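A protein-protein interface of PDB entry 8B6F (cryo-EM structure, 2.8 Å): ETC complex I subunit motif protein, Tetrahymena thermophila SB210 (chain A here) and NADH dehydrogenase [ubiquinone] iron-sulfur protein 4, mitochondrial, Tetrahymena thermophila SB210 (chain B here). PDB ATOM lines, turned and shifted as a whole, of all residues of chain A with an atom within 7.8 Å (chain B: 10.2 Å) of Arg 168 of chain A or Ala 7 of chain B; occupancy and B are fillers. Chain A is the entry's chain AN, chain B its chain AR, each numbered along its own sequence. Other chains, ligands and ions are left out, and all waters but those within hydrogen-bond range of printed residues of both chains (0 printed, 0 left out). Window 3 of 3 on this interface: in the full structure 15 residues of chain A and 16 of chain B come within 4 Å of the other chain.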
ATOM      1  N   GLU A 161     -11.309  19.965  33.797  1.00  0.00           N
ATOM      2  CA  GLU A 161     -11.587  19.459  32.457  1.00  0.00           C
ATOM      3  C   GLU A 161     -12.035  20.579  31.528  1.00  0.00           C
ATOM      4  O   GLU A 161     -11.609  20.642  30.369  1.00  0.00           O
ATOM      5  CB  GLU A 161     -12.646  18.359  32.526  1.00  0.00           C
ATOM      6  CG  GLU A 161     -12.997  17.744  31.177  1.00  0.00           C
ATOM      7  CD  GLU A 161     -11.798  17.120  30.490  1.00  0.00           C
ATOM      8  OE1 GLU A 161     -10.786  16.862  31.174  1.00  0.00           O
ATOM      9  OE2 GLU A 161     -11.867  16.890  29.265  1.00  0.00           O
ATOM     10  N   GLU A 162     -12.896  21.473  32.014  1.00  0.00           N
ATOM     11  CA  GLU A 162     -13.323  22.601  31.193  1.00  0.00           C
ATOM     12  C   GLU A 162     -12.147  23.508  30.855  1.00  0.00           C
ATOM     13  O   GLU A 162     -12.025  23.981  29.720  1.00  0.00           O
ATOM     14  CB  GLU A 162     -14.417  23.385  31.916  1.00  0.00           C
ATOM     15  CG  GLU A 162     -14.997  24.529  31.101  1.00  0.00           C
ATOM     16  CD  GLU A 162     -16.112  25.252  31.828  1.00  0.00           C
ATOM     17  OE1 GLU A 162     -16.383  24.904  32.996  1.00  0.00           O
ATOM     18  OE2 GLU A 162     -16.717  26.166  31.232  1.00  0.00           O
ATOM     19  N   GLN A 163     -11.268  23.763  31.828  1.00  0.00           N
ATOM     20  CA  GLN A 163     -10.090  24.579  31.559  1.00  0.00           C
ATOM     21  C   GLN A 163      -9.202  23.924  30.508  1.00  0.00           C
ATOM     22  O   GLN A 163      -8.697  24.597  29.603  1.00  0.00           O
ATOM     23  CB  GLN A 163      -9.310  24.816  32.853  1.00  0.00           C
ATOM     24  CG  GLN A 163      -8.058  25.674  32.693  1.00  0.00           C
ATOM     25  CD  GLN A 163      -8.366  27.090  32.242  1.00  0.00           C
ATOM     26  OE1 GLN A 163      -9.527  27.494  32.172  1.00  0.00           O
ATOM     27  NE2 GLN A 163      -7.323  27.854  31.935  1.00  0.00           N
ATOM     28  N   ASN A 164      -9.010  22.607  30.607  1.00  0.00           N
ATOM     29  CA  ASN A 164      -8.199  21.906  29.618  1.00  0.00           C
ATOM     30  C   ASN A 164      -8.836  21.983  28.237  1.00  0.00           C
ATOM     31  O   ASN A 164      -8.138  22.154  27.230  1.00  0.00           O
ATOM     32  CB  ASN A 164      -8.003  20.449  30.037  1.00  0.00           C
ATOM     33  CG  ASN A 164      -7.258  20.318  31.350  1.00  0.00           C
ATOM     34  OD1 ASN A 164      -6.480  21.193  31.725  1.00  0.00           O
ATOM     35  ND2 ASN A 164      -7.490  19.215  32.054  1.00  0.00           N
ATOM     36  N   GLU A 165     -10.163  21.859  28.169  1.00  0.00           N
ATOM     37  CA  GLU A 165     -10.849  21.998  26.890  1.00  0.00           C
ATOM     38  C   GLU A 165     -10.636  23.389  26.307  1.00  0.00           C
ATOM     39  O   GLU A 165     -10.384  23.534  25.106  1.00  0.00           O
ATOM     40  CB  GLU A 165     -12.340  21.706  27.071  1.00  0.00           C
ATOM     41  CG  GLU A 165     -13.232  22.207  25.941  1.00  0.00           C
ATOM     42  CD  GLU A 165     -12.813  21.685  24.583  1.00  0.00           C
ATOM     43  OE1 GLU A 165     -12.076  20.678  24.530  1.00  0.00           O
ATOM     44  OE2 GLU A 165     -13.222  22.285  23.567  1.00  0.00           O
ATOM     45  N   MET A 166     -10.738  24.424  27.142  1.00  0.00           N
ATOM     46  CA  MET A 166     -10.505  25.783  26.664  1.00  0.00           C
ATOM     47  C   MET A 166      -9.083  25.941  26.138  1.00  0.00           C
ATOM     48  O   MET A 166      -8.866  26.544  25.081  1.00  0.00           O
ATOM     49  CB  MET A 166     -10.784  26.780  27.791  1.00  0.00           C
ATOM     50  CG  MET A 166     -10.809  28.241  27.356  1.00  0.00           C
ATOM     51  SD  MET A 166      -9.181  28.978  27.100  1.00  0.00           S
ATOM     52  CE  MET A 166      -8.488  28.891  28.749  1.00  0.00           C
ATOM     53  N   ILE A 167      -8.098  25.420  26.873  1.00  0.00           N
ATOM     54  CA  ILE A 167      -6.707  25.523  26.439  1.00  0.00           C
ATOM     55  C   ILE A 167      -6.505  24.792  25.118  1.00  0.00           C
ATOM     56  O   ILE A 167      -5.825  25.291  24.213  1.00  0.00           O
ATOM     57  CB  ILE A 167      -5.762  24.987  27.532  1.00  0.00           C
ATOM     58  CG1 ILE A 167      -5.822  25.870  28.785  1.00  0.00           C
ATOM     59  CG2 ILE A 167      -4.328  24.886  27.011  1.00  0.00           C
ATOM     60  CD1 ILE A 167      -5.352  27.300  28.582  1.00  0.00           C
ATOM     61  N   ARG A 168      -7.084  23.598  24.987  1.00  0.00           N
ATOM     62  CA  ARG A 168      -6.930  22.832  23.754  1.00  0.00           C
ATOM     63  C   ARG A 168      -7.512  23.580  22.563  1.00  0.00           C
ATOM     64  O   ARG A 168      -6.876  23.682  21.508  1.00  0.00           O
ATOM     65  CB  ARG A 168      -7.598  21.464  23.904  1.00  0.00           C
ATOM     66  CG  ARG A 168      -7.410  20.548  22.700  1.00  0.00           C
ATOM     67  CD  ARG A 168      -8.372  19.372  22.735  1.00  0.00           C
ATOM     68  NE  ARG A 168      -9.763  19.800  22.633  1.00  0.00           N
ATOM     69  CZ  ARG A 168     -10.371  20.115  21.497  1.00  0.00           C
ATOM     70  NH1 ARG A 168      -9.734  20.075  20.337  1.00  0.00           N
ATOM     71  NH2 ARG A 168     -11.650  20.476  21.524  1.00  0.00           N
ATOM     72  N   ILE A 169      -8.725  24.115  22.711  1.00  0.00           N
ATOM     73  CA  ILE A 169      -9.359  24.788  21.583  1.00  0.00           C
ATOM     74  C   ILE A 169      -8.625  26.077  21.237  1.00  0.00           C
ATOM     75  O   ILE A 169      -8.625  26.505  20.077  1.00  0.00           O
ATOM     76  CB  ILE A 169     -10.849  25.044  21.880  1.00  0.00           C
ATOM     77  CG1 ILE A 169     -11.563  25.605  20.649  1.00  0.00           C
ATOM     78  CG2 ILE A 169     -11.015  25.998  23.050  1.00  0.00           C
ATOM     79  CD1 ILE A 169     -11.520  24.689  19.446  1.00  0.00           C
ATOM     80  N   ALA A 170      -7.996  26.719  22.222  1.00  0.00           N
ATOM     81  CA  ALA A 170      -7.264  27.951  21.958  1.00  0.00           C
ATOM     82  C   ALA A 170      -6.023  27.736  21.103  1.00  0.00           C
ATOM     83  O   ALA A 170      -5.453  28.720  20.621  1.00  0.00           O
ATOM     84  CB  ALA A 170      -6.862  28.609  23.279  1.00  0.00           C
ATOM     85  N   SER A 171      -5.585  26.493  20.910  1.00  0.00           N
ATOM     86  CA  SER A 171      -4.343  26.203  20.207  1.00  0.00           C
ATOM     87  C   SER A 171      -4.565  25.713  18.782  1.00  0.00           C
ATOM     88  O   SER A 171      -3.604  25.302  18.126  1.00  0.00           O
ATOM     89  CB  SER A 171      -3.528  25.168  20.986  1.00  0.00           C
ATOM     90  OG  SER A 171      -4.225  23.937  21.075  1.00  0.00           O
ATOM     91  N   GLN A 172      -5.800  25.742  18.288  1.00  0.00           N
ATOM     92  CA  GLN A 172      -6.087  25.237  16.956  1.00  0.00           C
ATOM     93  C   GLN A 172      -5.636  26.226  15.887  1.00  0.00           C
ATOM     94  O   GLN A 172      -5.627  27.441  16.097  1.00  0.00           O
ATOM     95  CB  GLN A 172      -7.585  24.959  16.799  1.00  0.00           C
ATOM     96  CG  GLN A 172      -8.140  23.954  17.795  1.00  0.00           C
ATOM     97  CD  GLN A 172      -7.511  22.582  17.657  1.00  0.00           C
ATOM     98  OE1 GLN A 172      -6.908  22.263  16.634  1.00  0.00           O
ATOM     99  NE2 GLN A 172      -7.646  21.762  18.693  1.00  0.00           N
ATOM    100  N   LYS A 173      -5.251  25.687  14.733  1.00  0.00           N
ATOM    101  CA  LYS A 173      -4.927  26.521  13.584  1.00  0.00           C
ATOM    102  C   LYS A 173      -6.189  27.190  13.048  1.00  0.00           C
ATOM    103  O   LYS A 173      -7.279  26.615  13.067  1.00  0.00           O
ATOM    104  CB  LYS A 173      -4.271  25.683  12.485  1.00  0.00           C
ATOM    105  CG  LYS A 173      -3.935  26.466  11.220  1.00  0.00           C
ATOM    106  CD  LYS A 173      -3.414  25.555  10.124  1.00  0.00           C
ATOM    107  CE  LYS A 173      -3.256  26.312   8.813  1.00  0.00           C
ATOM    108  NZ  LYS A 173      -2.847  25.418   7.693  1.00  0.00           N
ATOM    109  N   LEU B   2     -12.015  30.373  10.529  1.00  0.00           N
ATOM    110  CA  LEU B   2     -12.390  29.001  10.187  1.00  0.00           C
ATOM    111  C   LEU B   2     -11.513  28.058  11.001  1.00  0.00           C
ATOM    112  O   LEU B   2     -10.341  27.855  10.669  1.00  0.00           O
ATOM    113  CB  LEU B   2     -12.238  28.733   8.699  1.00  0.00           C
ATOM    114  CG  LEU B   2     -13.242  29.378   7.754  1.00  0.00           C
ATOM    115  CD1 LEU B   2     -12.836  28.992   6.357  1.00  0.00           C
ATOM    116  CD2 LEU B   2     -14.672  28.952   8.051  1.00  0.00           C
ATOM    117  N   LEU B   3     -12.082  27.489  12.055  1.00  0.00           N
ATOM    118  CA  LEU B   3     -11.381  26.477  12.816  1.00  0.00           C
ATOM    119  C   LEU B   3     -11.364  25.164  12.037  1.00  0.00           C
ATOM    120  O   LEU B   3     -12.153  24.972  11.110  1.00  0.00           O
ATOM    121  CB  LEU B   3     -12.041  26.284  14.176  1.00  0.00           C
ATOM    122  CG  LEU B   3     -11.687  27.335  15.232  1.00  0.00           C
ATOM    123  CD1 LEU B   3     -12.138  28.730  14.818  1.00  0.00           C
ATOM    124  CD2 LEU B   3     -12.290  26.953  16.565  1.00  0.00           C
ATOM    125  N   PRO B   4     -10.468  24.244  12.391  1.00  0.00           N
ATOM    126  CA  PRO B   4     -10.376  22.988  11.640  1.00  0.00           C
ATOM    127  C   PRO B   4     -11.694  22.233  11.666  1.00  0.00           C
ATOM    128  O   PRO B   4     -12.457  22.303  12.631  1.00  0.00           O
ATOM    129  CB  PRO B   4      -9.268  22.215  12.367  1.00  0.00           C
ATOM    130  CG  PRO B   4      -8.495  23.253  13.110  1.00  0.00           C
ATOM    131  CD  PRO B   4      -9.496  24.294  13.495  1.00  0.00           C
ATOM    132  N   LYS B   5     -11.964  21.515  10.577  1.00  0.00           N
ATOM    133  CA  LYS B   5     -13.229  20.807  10.452  1.00  0.00           C
ATOM    134  C   LYS B   5     -13.440  19.877  11.640  1.00  0.00           C
ATOM    135  O   LYS B   5     -12.516  19.194  12.090  1.00  0.00           O
ATOM    136  CB  LYS B   5     -13.264  20.009   9.147  1.00  0.00           C
ATOM    137  CG  LYS B   5     -14.558  19.237   8.935  1.00  0.00           C
ATOM    138  CD  LYS B   5     -14.583  18.550   7.579  1.00  0.00           C
ATOM    139  CE  LYS B   5     -15.861  17.746   7.392  1.00  0.00           C
ATOM    140  NZ  LYS B   5     -17.082  18.593   7.522  1.00  0.00           N
ATOM    141  N   ASN B   6     -14.672  19.871  12.155  1.00  0.00           N
ATOM    142  CA  ASN B   6     -15.058  19.057  13.311  1.00  0.00           C
ATOM    143  C   ASN B   6     -14.054  19.190  14.452  1.00  0.00           C
ATOM    144  O   ASN B   6     -13.837  18.251  15.222  1.00  0.00           O
ATOM    145  CB  ASN B   6     -15.244  17.586  12.921  1.00  0.00           C
ATOM    146  CG  ASN B   6     -13.942  16.905  12.555  1.00  0.00           C
ATOM    147  OD1 ASN B   6     -13.558  16.863  11.386  1.00  0.00           O
ATOM    148  ND2 ASN B   6     -13.254  16.367  13.554  1.00  0.00           N
ATOM    149  N   ALA B   7     -13.428  20.364  14.566  1.00  0.00           N
ATOM    150  CA  ALA B   7     -12.545  20.620  15.699  1.00  0.00           C
ATOM    151  C   ALA B   7     -13.335  20.715  16.997  1.00  0.00           C
ATOM    152  O   ALA B   7     -12.881  20.237  18.043  1.00  0.00           O
ATOM    153  CB  ALA B   7     -11.742  21.898  15.463  1.00  0.00           C
ATOM    154  N   ILE B   8     -14.513  21.331  16.950  1.00  0.00           N
ATOM    155  CA  ILE B   8     -15.403  21.445  18.099  1.00  0.00           C
ATOM    156  C   ILE B   8     -16.622  20.575  17.836  1.00  0.00           C
ATOM    157  O   ILE B   8     -17.266  20.700  16.787  1.00  0.00           O
ATOM    158  CB  ILE B   8     -15.822  22.905  18.351  1.00  0.00           C
ATOM    159  CG1 ILE B   8     -14.594  23.819  18.348  1.00  0.00           C
ATOM    160  CG2 ILE B   8     -16.572  23.008  19.674  1.00  0.00           C
ATOM    161  CD1 ILE B   8     -14.909  25.286  18.552  1.00  0.00           C
ATOM    162  N   GLN B   9     -16.935  19.696  18.782  1.00  0.00           N
ATOM    163  CA  GLN B   9     -18.070  18.788  18.676  1.00  0.00           C
ATOM    164  C   GLN B   9     -18.884  18.806  19.961  1.00  0.00           C
ATOM    165  O   GLN B   9     -19.374  17.774  20.426  1.00  0.00           O
ATOM    166  CB  GLN B   9     -17.605  17.373  18.348  1.00  0.00           C
ATOM    167  CG  GLN B   9     -16.816  17.278  17.048  1.00  0.00           C
ATOM    168  CD  GLN B   9     -16.418  15.853  16.701  1.00  0.00           C
ATOM    169  OE1 GLN B   9     -16.452  15.458  15.536  1.00  0.00           O
ATOM    170  NE2 GLN B   9     -16.032  15.078  17.710  1.00  0.00           N
ATOM    171  N   SER B  10     -19.039  19.986  20.552  1.00  0.00           N
ATOM    172  CA  SER B  10     -19.774  20.123  21.798  1.00  0.00           C
ATOM    173  C   SER B  10     -21.270  20.232  21.532  1.00  0.00           C
ATOM    174  O   SER B  10     -21.705  20.660  20.460  1.00  0.00           O
ATOM    175  CB  SER B  10     -19.299  21.354  22.570  1.00  0.00           C
ATOM    176  OG  SER B  10     -17.922  21.253  22.890  1.00  0.00           O
ATOM    177  N   TYR B  13     -22.131  23.751  20.870  1.00  0.00           N
ATOM    178  CA  TYR B  13     -21.782  24.131  19.506  1.00  0.00           C
ATOM    179  C   TYR B  13     -22.828  23.636  18.513  1.00  0.00           C
ATOM    180  O   TYR B  13     -23.234  24.375  17.609  1.00  0.00           O
ATOM    181  CB  TYR B  13     -20.401  23.573  19.161  1.00  0.00           C
ATOM    182  CG  TYR B  13     -19.821  24.082  17.864  1.00  0.00           C
ATOM    183  CD1 TYR B  13     -19.300  25.366  17.767  1.00  0.00           C
ATOM    184  CD2 TYR B  13     -19.768  23.267  16.743  1.00  0.00           C
ATOM    185  CE1 TYR B  13     -18.758  25.829  16.583  1.00  0.00           C
ATOM    186  CE2 TYR B  13     -19.229  23.720  15.555  1.00  0.00           C
ATOM    187  CZ  TYR B  13     -18.725  25.000  15.480  1.00  0.00           C
ATOM    188  OH  TYR B  13     -18.188  25.451  14.297  1.00  0.00           O
ATOM    189  N   PHE B  14     -23.275  22.389  18.664  1.00  0.00           N
ATOM    190  CA  PHE B  14     -24.302  21.860  17.772  1.00  0.00           C
ATOM    191  C   PHE B  14     -25.615  22.613  17.939  1.00  0.00           C
ATOM    192  O   PHE B  14     -26.323  22.869  16.959  1.00  0.00           O
ATOM    193  CB  PHE B  14     -24.501  20.364  18.024  1.00  0.00           C
ATOM    194  CG  PHE B  14     -23.290  19.528  17.710  1.00  0.00           C
ATOM    195  CD1 PHE B  14     -22.415  19.892  16.698  1.00  0.00           C
ATOM    196  CD2 PHE B  14     -23.029  18.374  18.431  1.00  0.00           C
ATOM    197  CE1 PHE B  14     -21.304  19.123  16.411  1.00  0.00           C
ATOM    198  CE2 PHE B  14     -21.918  17.600  18.148  1.00  0.00           C
ATOM    199  CZ  PHE B  14     -21.055  17.975  17.137  1.00  0.00           C
ATOM    200  N   GLN B  17     -25.340  25.830  16.071  1.00  0.00           N
ATOM    201  CA  GLN B  17     -25.486  25.605  14.637  1.00  0.00           C
ATOM    202  C   GLN B  17     -26.944  25.390  14.253  1.00  0.00           C
ATOM    203  O   GLN B  17     -27.422  25.955  13.263  1.00  0.00           O
ATOM    204  CB  GLN B  17     -24.640  24.407  14.210  1.00  0.00           C
ATOM    205  CG  GLN B  17     -23.149  24.696  14.142  1.00  0.00           C
ATOM    206  CD  GLN B  17     -22.368  23.547  13.542  1.00  0.00           C
ATOM    207  OE1 GLN B  17     -22.852  22.418  13.480  1.00  0.00           O
ATOM    208  NE2 GLN B  17     -21.152  23.830  13.091  1.00  0.00           N
ATOM    209  N   GLN B  50     -19.928  27.097   5.618  1.00  0.00           N
ATOM    210  CA  GLN B  50     -19.923  26.461   4.307  1.00  0.00           C
ATOM    211  C   GLN B  50     -21.283  26.509   3.625  1.00  0.00           C
ATOM    212  O   GLN B  50     -21.395  26.068   2.476  1.00  0.00           O
ATOM    213  CB  GLN B  50     -19.463  25.004   4.427  1.00  0.00           C
ATOM    214  CG  GLN B  50     -17.973  24.841   4.704  1.00  0.00           C
ATOM    215  CD  GLN B  50     -17.570  25.320   6.087  1.00  0.00           C
ATOM    216  OE1 GLN B  50     -18.414  25.516   6.959  1.00  0.00           O
ATOM    217  NE2 GLN B  50     -16.272  25.516   6.288  1.00  0.00           N
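Of the 13 printed residues of chain B, 4 touch a printed residue of chain A.
Printed residues of chain B that touch a printed residue of chain A: Leu 3, Pro 4, Ala 7 and Ile 8.
Hydrophobic or aromatic side chains of chain B that line the printed part of chain A: Leu 3, Pro 4 and Ile 8.
Along chain B the printed residues that touch a printed residue of chain A span positions 3 to 8.
Printed residues of chain A that touch a printed residue of chain B: Arg 168, Ile 169, Gln 172 and Lys 173.
Along chain A the printed residues that touch a printed residue of chain B span positions 168 to 173.
Among the printed residues, 5 pairs touch across the chains.
Among the printed residues, no Asp or Glu carboxylate lies within 4 Å of a Lys or Arg side-chain nitrogen of the other chain.
Arg 168 of chain A touches one residue of chain B.
Of chain A, only Arg 168 comes within 4 Å of Ala 7 of chain B.
Glu 165 of chain A touches none of the printed residues of chain B.
No residue of chain B comes within 4 Å of Ile 167 of chain A.
Ile 169 of chain A touches just these residues of chain B: Leu 3 and Ile 8.
No residue of chain B comes within 4 Å of Ala 170 of chain A.
Ser 171 of chain A touches none of the printed residues of chain B.
Printed residues of chain B within 4 Å of Lys 173 of chain A: Pro 4.
Printed residues of chain A within 4 Å of Leu 3 of chain B: Ile 169.
Of the printed residues of chain A, Pro 4 of chain B touches Gln 172 and Lys 173.
Of the printed residues of chain B, Gln 172 of chain A touches Pro 4.
Met 166 of chain A touches none of the printed residues of chain B.
The nearest residue of chain B that does not touch Arg 168 of chain A is Ile 8 of chain B (5.2 Å).
The nearest residue of chain A that does not touch Ala 7 of chain B is Gln 172 of chain A (4.8 Å).
The nearest printed residue of chain B that does not touch Lys 173 of chain A is Leu 2 of chain B (4.1 Å).
NH2 of Arg 168 of chain A touches O of Ala 7 of chain B, 3.7 Å away.
Leu 3 of chain B touches Ile 169 of chain A (CD2 to CD1, 3.7 Å).
Ile 8 of chain B touches Ile 169 of chain A.
CD of Pro 4 of chain B touches CB of Gln 172 of chain A (3.9 Å).
O of Lys 173 of chain A touches CD of Pro 4 of chain B, 3.2 Å away.
The side-chain amide nitrogen of Gln 172 of chain A lies close to the guanidinium group of Arg 168 of chain A (3.1 Å).
OG of Ser 171 of chain A lies within hydrogen-bond range of O of Arg 168 of chain A (2.7 Å).
The side-chain carboxylate (OE1) of Glu 165 of chain A lies within salt-bridge range of the guanidinium group (NH2) of Arg 168 of chain A, 3.0 Å away.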
